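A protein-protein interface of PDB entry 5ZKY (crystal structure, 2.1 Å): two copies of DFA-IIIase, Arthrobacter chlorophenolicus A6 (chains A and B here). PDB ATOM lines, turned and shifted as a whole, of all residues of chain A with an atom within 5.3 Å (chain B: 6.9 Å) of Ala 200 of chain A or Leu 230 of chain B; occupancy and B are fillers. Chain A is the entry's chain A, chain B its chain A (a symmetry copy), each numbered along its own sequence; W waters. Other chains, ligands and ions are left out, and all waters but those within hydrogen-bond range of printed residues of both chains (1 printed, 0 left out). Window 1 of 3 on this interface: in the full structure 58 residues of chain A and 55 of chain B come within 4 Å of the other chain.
OG of Ser 178 of chain A is in hydrogen-bond range of NE2 of His 78 of chain B (2.7 Å).
NE2 of His 205 of chain B sits at hydrogen-bond distance from OG of Ser 202 of chain A, 2.7 Å away.
The side-chain amide nitrogen (ND2) of Asn 254 of chain B sits at hydrogen-bond distance from the backbone carbonyl oxygen (O) of Ser 224 of chain A, 3.1 Å away.
The side-chain amino group of Lys 225 of chain A is in salt-bridge range of the side-chain carboxylate of Asp 228 of chain B (2.7 Å).
No position is printed for both chains.
Of the 15 pairs that touch across the chains among the printed residues, none has its exchanged pair printed and touching as well.
Water W1 lies within hydrogen-bond range of O of Asn 206 of chain B (3.0 Å), NZ of Lys 225 of chain A (3.1 Å) and O of Asp 228 of chain B (3.3 Å).
Hydrophobic or aromatic side chains of chain A that line the printed part of chain B: Ala 200 and Ala 223.
Printed residues of chain B that touch a printed residue of chain A: His 78, Phe 80, His 205, Phe 207, Asp 228, Asn 229, Leu 230, Asn 254 and Arg 277.
Hydrophobic or aromatic side chains of chain B within 4 Å of the printed part of chain A: His 78, Phe 80, His 205, Phe 207 and Leu 230.
Among the printed residues, 15 pairs touch across the chains.
Among the printed residues, Asp or Glu carboxylates within 4 Å of a Lys or Arg side-chain nitrogen of the other chain: Lys 225 of chain A with Asp 228 of chain B.
Ser 178 of chain A touches Phe 80 of chain B (OG to CB, 3.7 Å).
OG of Ser 178 of chain A touches CD2 of Phe 207 of chain B (3.1 Å).
Ala 200 of chain A touches Phe 207 of chain B (O to CE2, 3.6 Å).
Ala 200 of chain A touches Leu 230 of chain B.
O of Ala 223 of chain A touches CD2 of Leu 230 of chain B (3.2 Å).
ND2 of Asn 254 of chain B touches C of Ala 223 of chain A (3.4 Å).
Ala 223 of chain A touches Arg 277 of chain B (CB to NH1, 3.8 Å).
NZ of Lys 225 of chain A touches CD2 of His 205 of chain B, at 3.3 Å.
Lys 225 of chain A touches Asn 229 of chain B.
CG of Leu 230 of chain B touches CE of Lys 225 of chain A, 3.8 Å away.
The backbone carbonyl oxygen of Phe 179 of chain A is in hydrogen-bond range of the backbone NH of Ser 202 of chain A (3.0 Å).
The side-chain hydroxyl (OG) of Ser 224 of chain A lies within hydrogen-bond range of the backbone NH (N) of Leu 201 of chain A (3.2 Å).
The backbone NH (N) of His 205 of chain B lies close to the backbone carbonyl oxygen (O) of Asp 228 of chain B (3.5 Å).
The side-chain amide oxygen of Asn 229 of chain B lies within hydrogen-bond range of the backbone NH of His 205 of chain B, at 3.4 Å.
The backbone NH (N) of Asn 254 of chain B sits at hydrogen-bond distance from the backbone carbonyl oxygen (O) of Asn 229 of chain B (2.9 Å).
The backbone NH (N) of Arg 277 of chain B lies within hydrogen-bond range of the backbone carbonyl oxygen (O) of Asn 253 of chain B, at 2.9 Å.
Ala 200 of chain A touches just these residues of chain B: Phe 207 and Leu 230.
Leu 230 of chain B touches three residues of chain A.
Printed residues of chain A within 4 Å of Asn 254 of chain B: Ala 223 and Ser 224.
Printed residues of chain A within 4 Å of Asp 228 of chain B: Lys 225 (2.7 Å).
The nearest residue of chain B that does not touch Ala 200 of chain A is Phe 256 of chain B (4.7 Å).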
ATOM      1  N   ASP A 177      -7.045  -1.835  12.501  1.00  0.00           N
ATOM      2  CA  ASP A 177      -8.148  -2.646  13.010  1.00  0.00           C
ATOM      3  C   ASP A 177      -9.369  -2.454  12.116  1.00  0.00           C
ATOM      4  O   ASP A 177      -9.680  -1.322  11.744  1.00  0.00           O
ATOM      5  CB  ASP A 177      -8.478  -2.195  14.441  1.00  0.00           C
ATOM      6  CG  ASP A 177      -9.406  -3.144  15.171  1.00  0.00           C
ATOM      7  OD1 ASP A 177      -9.428  -4.344  14.875  1.00  0.00           O
ATOM      8  OD2 ASP A 177     -10.112  -2.681  16.074  1.00  0.00           O
ATOM      9  N   SER A 178     -10.054  -3.550  11.777  1.00  0.00           N
ATOM     10  CA  SER A 178     -11.362  -3.513  11.071  1.00  0.00           C
ATOM     11  C   SER A 178     -11.298  -2.846   9.676  1.00  0.00           C
ATOM     12  O   SER A 178     -12.273  -2.237   9.223  1.00  0.00           O
ATOM     13  CB  SER A 178     -12.403  -2.832  11.965  1.00  0.00           C
ATOM     14  OG  SER A 178     -13.729  -3.156  11.611  1.00  0.00           O
ATOM     15  N   PHE A 179     -10.145  -2.966   9.001  1.00  0.00           N
ATOM     16  CA  PHE A 179     -10.007  -2.497   7.617  1.00  0.00           C
ATOM     17  C   PHE A 179     -10.796  -3.422   6.682  1.00  0.00           C
ATOM     18  O   PHE A 179     -11.021  -4.605   6.978  1.00  0.00           O
ATOM     19  CB  PHE A 179      -8.529  -2.423   7.176  1.00  0.00           C
ATOM     20  CG  PHE A 179      -7.834  -1.114   7.506  1.00  0.00           C
ATOM     21  CD1 PHE A 179      -8.149  -0.374   8.650  1.00  0.00           C
ATOM     22  CD2 PHE A 179      -6.845  -0.627   6.664  1.00  0.00           C
ATOM     23  CE1 PHE A 179      -7.507   0.822   8.929  1.00  0.00           C
ATOM     24  CE2 PHE A 179      -6.192   0.568   6.938  1.00  0.00           C
ATOM     25  CZ  PHE A 179      -6.524   1.293   8.071  1.00  0.00           C
ATOM     26  N   ALA A 198      -2.076  -6.107  10.751  1.00  0.00           N
ATOM     27  CA  ALA A 198      -3.519  -6.076  10.517  1.00  0.00           C
ATOM     28  C   ALA A 198      -4.301  -6.879  11.545  1.00  0.00           C
ATOM     29  O   ALA A 198      -4.071  -8.083  11.676  1.00  0.00           O
ATOM     30  CB  ALA A 198      -3.814  -6.624   9.132  1.00  0.00           C
ATOM     31  N   ASP A 199      -5.232  -6.214  12.246  1.00  0.00           N
ATOM     32  CA  ASP A 199      -6.196  -6.880  13.134  1.00  0.00           C
ATOM     33  C   ASP A 199      -7.594  -6.835  12.550  1.00  0.00           C
ATOM     34  O   ASP A 199      -8.055  -5.784  12.077  1.00  0.00           O
ATOM     35  CB  ASP A 199      -6.206  -6.244  14.526  1.00  0.00           C
ATOM     36  CG  ASP A 199      -4.901  -6.429  15.243  1.00  0.00           C
ATOM     37  OD1 ASP A 199      -4.327  -7.536  15.128  1.00  0.00           O
ATOM     38  OD2 ASP A 199      -4.447  -5.473  15.919  1.00  0.00           O
ATOM     39  N   ALA A 200      -8.255  -7.992  12.565  1.00  0.00           N
ATOM     40  CA  ALA A 200      -9.654  -8.100  12.170  1.00  0.00           C
ATOM     41  C   ALA A 200      -9.936  -7.414  10.820  1.00  0.00           C
ATOM     42  O   ALA A 200     -10.935  -6.714  10.633  1.00  0.00           O
ATOM     43  CB  ALA A 200     -10.533  -7.570  13.287  1.00  0.00           C
ATOM     44  N   LEU A 201      -9.015  -7.661   9.893  1.00  0.00           N
ATOM     45  CA  LEU A 201      -9.084  -7.212   8.511  1.00  0.00           C
ATOM     46  C   LEU A 201      -9.939  -8.160   7.679  1.00  0.00           C
ATOM     47  O   LEU A 201      -9.904  -9.376   7.879  1.00  0.00           O
ATOM     48  CB  LEU A 201      -7.667  -7.194   7.924  1.00  0.00           C
ATOM     49  CG  LEU A 201      -7.470  -7.162   6.418  1.00  0.00           C
ATOM     50  CD1 LEU A 201      -7.806  -5.787   5.873  1.00  0.00           C
ATOM     51  CD2 LEU A 201      -6.023  -7.519   6.142  1.00  0.00           C
ATOM     52  N   SER A 202     -10.682  -7.598   6.728  1.00  0.00           N
ATOM     53  CA  SER A 202     -11.386  -8.391   5.728  1.00  0.00           C
ATOM     54  C   SER A 202     -10.990  -7.973   4.313  1.00  0.00           C
ATOM     55  O   SER A 202     -11.235  -6.831   3.903  1.00  0.00           O
ATOM     56  CB  SER A 202     -12.895  -8.292   5.897  1.00  0.00           C
ATOM     57  OG  SER A 202     -13.518  -9.168   4.965  1.00  0.00           O
ATOM     58  N   GLN A 222      -3.882 -10.524  13.477  1.00  0.00           N
ATOM     59  CA  GLN A 222      -4.802 -11.404  14.193  1.00  0.00           C
ATOM     60  C   GLN A 222      -6.194 -11.325  13.620  1.00  0.00           C
ATOM     61  O   GLN A 222      -6.608 -10.271  13.141  1.00  0.00           O
ATOM     62  CB  GLN A 222      -4.941 -10.990  15.660  1.00  0.00           C
ATOM     63  CG  GLN A 222      -3.749 -11.303  16.499  1.00  0.00           C
ATOM     64  CD  GLN A 222      -3.486 -12.782  16.628  1.00  0.00           C
ATOM     65  OE1 GLN A 222      -2.335 -13.196  16.548  1.00  0.00           O
ATOM     66  NE2 GLN A 222      -4.538 -13.583  16.828  1.00  0.00           N
ATOM     67  N   ALA A 223      -6.906 -12.445  13.724  1.00  0.00           N
ATOM     68  CA  ALA A 223      -8.348 -12.496  13.516  1.00  0.00           C
ATOM     69  C   ALA A 223      -8.802 -11.917  12.171  1.00  0.00           C
ATOM     70  O   ALA A 223      -9.869 -11.337  12.087  1.00  0.00           O
ATOM     71  CB  ALA A 223      -9.050 -11.771  14.658  1.00  0.00           C
ATOM     72  N   SER A 224      -7.997 -12.097  11.127  1.00  0.00           N
ATOM     73  CA  SER A 224      -8.301 -11.532   9.827  1.00  0.00           C
ATOM     74  C   SER A 224      -8.844 -12.595   8.863  1.00  0.00           C
ATOM     75  O   SER A 224      -8.828 -13.805   9.147  1.00  0.00           O
ATOM     76  CB  SER A 224      -7.055 -10.856   9.259  1.00  0.00           C
ATOM     77  OG  SER A 224      -6.674  -9.777  10.100  1.00  0.00           O
ATOM     78  N   LYS A 225      -9.346 -12.141   7.722  1.00  0.00           N
ATOM     79  CA  LYS A 225      -9.842 -13.068   6.722  1.00  0.00           C
ATOM     80  C   LYS A 225      -9.663 -12.569   5.298  1.00  0.00           C
ATOM     81  O   LYS A 225      -9.711 -11.365   5.028  1.00  0.00           O
ATOM     82  CB  LYS A 225     -11.295 -13.469   7.003  1.00  0.00           C
ATOM     83  CG  LYS A 225     -12.310 -12.359   6.989  1.00  0.00           C
ATOM     84  CD  LYS A 225     -13.688 -12.898   7.351  1.00  0.00           C
ATOM     85  CE  LYS A 225     -14.683 -11.773   7.569  1.00  0.00           C
ATOM     86  NZ  LYS A 225     -15.171 -11.122   6.327  1.00  0.00           N
ATOM     87  N   HIS B  78     -18.681   1.371   8.005  1.00  0.00           N
ATOM     88  CA  HIS B  78     -18.999   0.548   9.178  1.00  0.00           C
ATOM     89  C   HIS B  78     -18.461   1.143  10.496  1.00  0.00           C
ATOM     90  O   HIS B  78     -18.965   0.840  11.578  1.00  0.00           O
ATOM     91  CB  HIS B  78     -18.578  -0.912   8.957  1.00  0.00           C
ATOM     92  CG  HIS B  78     -17.110  -1.188   9.093  1.00  0.00           C
ATOM     93  ND1 HIS B  78     -16.195  -0.871   8.110  1.00  0.00           N
ATOM     94  CD2 HIS B  78     -16.412  -1.830  10.062  1.00  0.00           C
ATOM     95  CE1 HIS B  78     -14.997  -1.290   8.477  1.00  0.00           C
ATOM     96  NE2 HIS B  78     -15.100  -1.882   9.654  1.00  0.00           N
ATOM     97  N   PHE B  80     -16.176   1.082  12.794  1.00  0.00           N
ATOM     98  CA  PHE B  80     -15.771   0.457  14.047  1.00  0.00           C
ATOM     99  C   PHE B  80     -14.434   0.980  14.571  1.00  0.00           C
ATOM    100  O   PHE B  80     -13.455   1.115  13.833  1.00  0.00           O
ATOM    101  CB  PHE B  80     -15.676  -1.056  13.906  1.00  0.00           C
ATOM    102  CG  PHE B  80     -15.332  -1.746  15.196  1.00  0.00           C
ATOM    103  CD1 PHE B  80     -16.333  -2.121  16.074  1.00  0.00           C
ATOM    104  CD2 PHE B  80     -14.005  -1.963  15.551  1.00  0.00           C
ATOM    105  CE1 PHE B  80     -16.028  -2.733  17.272  1.00  0.00           C
ATOM    106  CE2 PHE B  80     -13.689  -2.577  16.754  1.00  0.00           C
ATOM    107  CZ  PHE B  80     -14.701  -2.959  17.620  1.00  0.00           C
ATOM    108  N   HIS B 205     -20.855 -10.484   5.791  1.00  0.00           N
ATOM    109  CA  HIS B 205     -19.731  -9.542   5.752  1.00  0.00           C
ATOM    110  C   HIS B 205     -19.922  -8.323   6.654  1.00  0.00           C
ATOM    111  O   HIS B 205     -19.633  -7.188   6.267  1.00  0.00           O
ATOM    112  CB  HIS B 205     -19.398  -9.129   4.293  1.00  0.00           C
ATOM    113  CG  HIS B 205     -18.012  -8.574   4.140  1.00  0.00           C
ATOM    114  ND1 HIS B 205     -17.760  -7.225   4.005  1.00  0.00           N
ATOM    115  CD2 HIS B 205     -16.800  -9.184   4.193  1.00  0.00           C
ATOM    116  CE1 HIS B 205     -16.449  -7.034   3.937  1.00  0.00           C
ATOM    117  NE2 HIS B 205     -15.843  -8.205   4.058  1.00  0.00           N
ATOM    118  N   ASN B 206     -20.407  -8.567   7.867  1.00  0.00           N
ATOM    119  CA  ASN B 206     -20.536  -7.538   8.872  1.00  0.00           C
ATOM    120  C   ASN B 206     -19.356  -7.603   9.847  1.00  0.00           C
ATOM    121  O   ASN B 206     -18.566  -8.576   9.864  1.00  0.00           O
ATOM    122  CB  ASN B 206     -21.862  -7.700   9.628  1.00  0.00           C
ATOM    123  CG  ASN B 206     -23.059  -7.654   8.705  1.00  0.00           C
ATOM    124  OD1 ASN B 206     -23.456  -6.582   8.263  1.00  0.00           O
ATOM    125  ND2 ASN B 206     -23.638  -8.817   8.410  1.00  0.00           N
ATOM    126  N   PHE B 207     -19.233  -6.531  10.631  1.00  0.00           N
ATOM    127  CA  PHE B 207     -18.287  -6.447  11.737  1.00  0.00           C
ATOM    128  C   PHE B 207     -19.134  -6.173  12.963  1.00  0.00           C
ATOM    129  O   PHE B 207     -19.685  -5.096  13.091  1.00  0.00           O
ATOM    130  CB  PHE B 207     -17.283  -5.323  11.508  1.00  0.00           C
ATOM    131  CG  PHE B 207     -16.058  -5.434  12.370  1.00  0.00           C
ATOM    132  CD1 PHE B 207     -16.071  -4.983  13.684  1.00  0.00           C
ATOM    133  CD2 PHE B 207     -14.914  -6.036  11.882  1.00  0.00           C
ATOM    134  CE1 PHE B 207     -14.944  -5.108  14.490  1.00  0.00           C
ATOM    135  CE2 PHE B 207     -13.790  -6.166  12.673  1.00  0.00           C
ATOM    136  CZ  PHE B 207     -13.801  -5.694  13.984  1.00  0.00           C
ATOM    137  N   ILE B 208     -19.263  -7.167  13.840  1.00  0.00           N
ATOM    138  CA  ILE B 208     -20.218  -7.130  14.955  1.00  0.00           C
ATOM    139  C   ILE B 208     -19.436  -7.479  16.210  1.00  0.00           C
ATOM    140  O   ILE B 208     -19.199  -8.665  16.515  1.00  0.00           O
ATOM    141  CB  ILE B 208     -21.382  -8.131  14.766  1.00  0.00           C
ATOM    142  CG1 ILE B 208     -21.839  -8.168  13.289  1.00  0.00           C
ATOM    143  CG2 ILE B 208     -22.549  -7.766  15.694  1.00  0.00           C
ATOM    144  CD1 ILE B 208     -23.020  -9.066  13.025  1.00  0.00           C
ATOM    145  N   ALA B 209     -19.001  -6.444  16.923  1.00  0.00           N
ATOM    146  CA  ALA B 209     -18.029  -6.648  17.979  1.00  0.00           C
ATOM    147  C   ALA B 209     -18.253  -5.751  19.170  1.00  0.00           C
ATOM    148  O   ALA B 209     -18.863  -4.692  19.062  1.00  0.00           O
ATOM    149  CB  ALA B 209     -16.629  -6.472  17.436  1.00  0.00           C
ATOM    150  N   CYS B 214     -24.136 -10.728  19.812  1.00  0.00           N
ATOM    151  CA  CYS B 214     -24.015 -10.224  18.456  1.00  0.00           C
ATOM    152  C   CYS B 214     -25.234 -10.624  17.625  1.00  0.00           C
ATOM    153  O   CYS B 214     -26.176  -9.835  17.527  1.00  0.00           O
ATOM    154  CB  CYS B 214     -22.669 -10.654  17.878  1.00  0.00           C
ATOM    155  SG  CYS B 214     -21.333  -9.887  18.825  1.00  0.00           S
ATOM    156  N   ILE B 215     -25.245 -11.850  17.091  1.00  0.00           N
ATOM    157  CA  ILE B 215     -26.322 -12.331  16.206  1.00  0.00           C
ATOM    158  C   ILE B 215     -27.210 -13.350  16.928  1.00  0.00           C
ATOM    159  O   ILE B 215     -26.726 -14.396  17.341  1.00  0.00           O
ATOM    160  CB  ILE B 215     -25.763 -13.014  14.938  1.00  0.00           C
ATOM    161  CG1 ILE B 215     -24.939 -12.026  14.104  1.00  0.00           C
ATOM    162  CG2 ILE B 215     -26.898 -13.587  14.090  1.00  0.00           C
ATOM    163  CD1 ILE B 215     -23.973 -12.693  13.126  1.00  0.00           C
ATOM    164  N   THR B 227     -22.727 -15.548   6.962  1.00  0.00           N
ATOM    165  CA  THR B 227     -21.471 -15.776   6.252  1.00  0.00           C
ATOM    166  C   THR B 227     -20.507 -14.602   6.287  1.00  0.00           C
ATOM    167  O   THR B 227     -20.917 -13.445   6.215  1.00  0.00           O
ATOM    168  CB  THR B 227     -21.722 -16.141   4.770  1.00  0.00           C
ATOM    169  OG1 THR B 227     -22.396 -15.060   4.107  1.00  0.00           O
ATOM    170  CG2 THR B 227     -22.550 -17.403   4.669  1.00  0.00           C
ATOM    171  N   ASP B 228     -19.216 -14.918   6.377  1.00  0.00           N
ATOM    172  CA  ASP B 228     -18.154 -13.942   6.179  1.00  0.00           C
ATOM    173  C   ASP B 228     -18.201 -12.777   7.173  1.00  0.00           C
ATOM    174  O   ASP B 228     -17.786 -11.662   6.846  1.00  0.00           O
ATOM    175  CB  ASP B 228     -18.169 -13.453   4.715  1.00  0.00           C
ATOM    176  CG  ASP B 228     -16.833 -13.597   4.059  1.00  0.00           C
ATOM    177  OD1 ASP B 228     -15.857 -12.948   4.499  1.00  0.00           O
ATOM    178  OD2 ASP B 228     -16.758 -14.370   3.100  1.00  0.00           O
ATOM    179  N   ASN B 229     -18.685 -13.043   8.389  1.00  0.00           N
ATOM    180  CA  ASN B 229     -18.740 -12.034   9.435  1.00  0.00           C
ATOM    181  C   ASN B 229     -17.526 -12.091  10.358  1.00  0.00           C
ATOM    182  O   ASN B 229     -16.936 -13.156  10.567  1.00  0.00           O
ATOM    183  CB  ASN B 229     -20.015 -12.168  10.271  1.00  0.00           C
ATOM    184  CG  ASN B 229     -21.260 -12.046   9.435  1.00  0.00           C
ATOM    185  OD1 ASN B 229     -21.665 -10.938   9.049  1.00  0.00           O
ATOM    186  ND2 ASN B 229     -21.862 -13.187   9.111  1.00  0.00           N
ATOM    187  N   LEU B 230     -17.176 -10.925  10.902  1.00  0.00           N
ATOM    188  CA  LEU B 230     -16.241 -10.812  12.011  1.00  0.00           C
ATOM    189  C   LEU B 230     -17.083 -10.539  13.244  1.00  0.00           C
ATOM    190  O   LEU B 230     -17.853  -9.584  13.256  1.00  0.00           O
ATOM    191  CB  LEU B 230     -15.246  -9.685  11.763  1.00  0.00           C
ATOM    192  CG  LEU B 230     -14.078 -10.139  10.898  1.00  0.00           C
ATOM    193  CD1 LEU B 230     -13.547  -8.978  10.051  1.00  0.00           C
ATOM    194  CD2 LEU B 230     -12.987 -10.741  11.768  1.00  0.00           C
ATOM    195  N   VAL B 231     -16.959 -11.397  14.256  1.00  0.00           N
ATOM    196  CA  VAL B 231     -17.883 -11.397  15.390  1.00  0.00           C
ATOM    197  C   VAL B 231     -17.140 -11.550  16.707  1.00  0.00           C
ATOM    198  O   VAL B 231     -16.318 -12.451  16.859  1.00  0.00           O
ATOM    199  CB  VAL B 231     -18.907 -12.553  15.303  1.00  0.00           C
ATOM    200  CG1 VAL B 231     -19.922 -12.463  16.445  1.00  0.00           C
ATOM    201  CG2 VAL B 231     -19.621 -12.546  13.959  1.00  0.00           C
ATOM    202  N   GLY B 232     -17.482 -10.693  17.667  1.00  0.00           N
ATOM    203  CA  GLY B 232     -16.954 -10.774  19.022  1.00  0.00           C
ATOM    204  C   GLY B 232     -17.949 -10.256  20.036  1.00  0.00           C
ATOM    205  O   GLY B 232     -18.354  -9.096  19.976  1.00  0.00           O
ATOM    206  N   ALA B 252     -17.591 -19.350   6.947  1.00  0.00           N
ATOM    207  CA  ALA B 252     -16.603 -18.294   6.637  1.00  0.00           C
ATOM    208  C   ALA B 252     -16.625 -17.142   7.648  1.00  0.00           C
ATOM    209  O   ALA B 252     -16.268 -16.047   7.286  1.00  0.00           O
ATOM    210  CB  ALA B 252     -16.774 -17.825   5.217  1.00  0.00           C
ATOM    211  N   ASN B 253     -17.058 -17.408   8.867  1.00  0.00           N
ATOM    212  CA  ASN B 253     -17.035 -16.407   9.912  1.00  0.00           C
ATOM    213  C   ASN B 253     -15.737 -16.538  10.694  1.00  0.00           C
ATOM    214  O   ASN B 253     -15.173 -17.620  10.823  1.00  0.00           O
ATOM    215  CB  ASN B 253     -18.238 -16.568  10.841  1.00  0.00           C
ATOM    216  CG  ASN B 253     -19.550 -16.429  10.108  1.00  0.00           C
ATOM    217  OD1 ASN B 253     -19.927 -15.320   9.696  1.00  0.00           O
ATOM    218  ND2 ASN B 253     -20.259 -17.564   9.924  1.00  0.00           N
ATOM    219  N   ASN B 254     -15.255 -15.406  11.181  1.00  0.00           N
ATOM    220  CA  ASN B 254     -14.115 -15.358  12.063  1.00  0.00           C
ATOM    221  C   ASN B 254     -14.679 -14.820  13.370  1.00  0.00           C
ATOM    222  O   ASN B 254     -14.954 -13.631  13.491  1.00  0.00           O
ATOM    223  CB  ASN B 254     -13.001 -14.468  11.498  1.00  0.00           C
ATOM    224  CG  ASN B 254     -11.685 -14.644  12.244  1.00  0.00           C
ATOM    225  OD1 ASN B 254     -11.679 -14.705  13.477  1.00  0.00           O
ATOM    226  ND2 ASN B 254     -10.561 -14.737  11.502  1.00  0.00           N
ATOM    227  N   VAL B 255     -14.884 -15.727  14.322  1.00  0.00           N
ATOM    228  CA  VAL B 255     -15.482 -15.404  15.609  1.00  0.00           C
ATOM    229  C   VAL B 255     -14.367 -15.380  16.634  1.00  0.00           C
ATOM    230  O   VAL B 255     -13.667 -16.391  16.842  1.00  0.00           O
ATOM    231  CB  VAL B 255     -16.549 -16.432  16.034  1.00  0.00           C
ATOM    232  CG1 VAL B 255     -17.210 -16.015  17.340  1.00  0.00           C
ATOM    233  CG2 VAL B 255     -17.604 -16.548  14.950  1.00  0.00           C
ATOM    234  N   PHE B 256     -14.203 -14.223  17.265  1.00  0.00           N
ATOM    235  CA  PHE B 256     -13.143 -14.022  18.240  1.00  0.00           C
ATOM    236  C   PHE B 256     -13.823 -13.756  19.588  1.00  0.00           C
ATOM    237  O   PHE B 256     -15.062 -13.672  19.649  1.00  0.00           O
ATOM    238  CB  PHE B 256     -12.137 -12.925  17.777  1.00  0.00           C
ATOM    239  CG  PHE B 256     -12.784 -11.659  17.287  1.00  0.00           C
ATOM    240  CD1 PHE B 256     -13.165 -10.672  18.177  1.00  0.00           C
ATOM    241  CD2 PHE B 256     -13.023 -11.465  15.926  1.00  0.00           C
ATOM    242  CE1 PHE B 256     -13.763  -9.508  17.720  1.00  0.00           C
ATOM    243  CE2 PHE B 256     -13.610 -10.302  15.468  1.00  0.00           C
ATOM    244  CZ  PHE B 256     -13.986  -9.320  16.363  1.00  0.00           C
ATOM    245  N   ARG B 277     -13.595 -19.955  11.615  1.00  0.00           N
ATOM    246  CA  ARG B 277     -12.501 -19.853  12.548  1.00  0.00           C
ATOM    247  C   ARG B 277     -13.141 -19.353  13.824  1.00  0.00           C
ATOM    248  O   ARG B 277     -13.790 -18.307  13.815  1.00  0.00           O
ATOM    249  CB  ARG B 277     -11.429 -18.884  12.025  1.00  0.00           C
ATOM    250  CG  ARG B 277     -10.219 -18.751  12.940  1.00  0.00           C
ATOM    251  CD  ARG B 277     -10.395 -17.610  13.928  1.00  0.00           C
ATOM    252  NE  ARG B 277      -9.355 -17.581  14.949  1.00  0.00           N
ATOM    253  CZ  ARG B 277      -9.042 -16.520  15.694  1.00  0.00           C
ATOM    254  NH1 ARG B 277      -9.686 -15.359  15.569  1.00  0.00           N
ATOM    255  NH2 ARG B 277      -8.062 -16.622  16.587  1.00  0.00           N
HETATM  256  O   HOH W   1     -16.646  -8.691   7.566  1.00  0.00           O
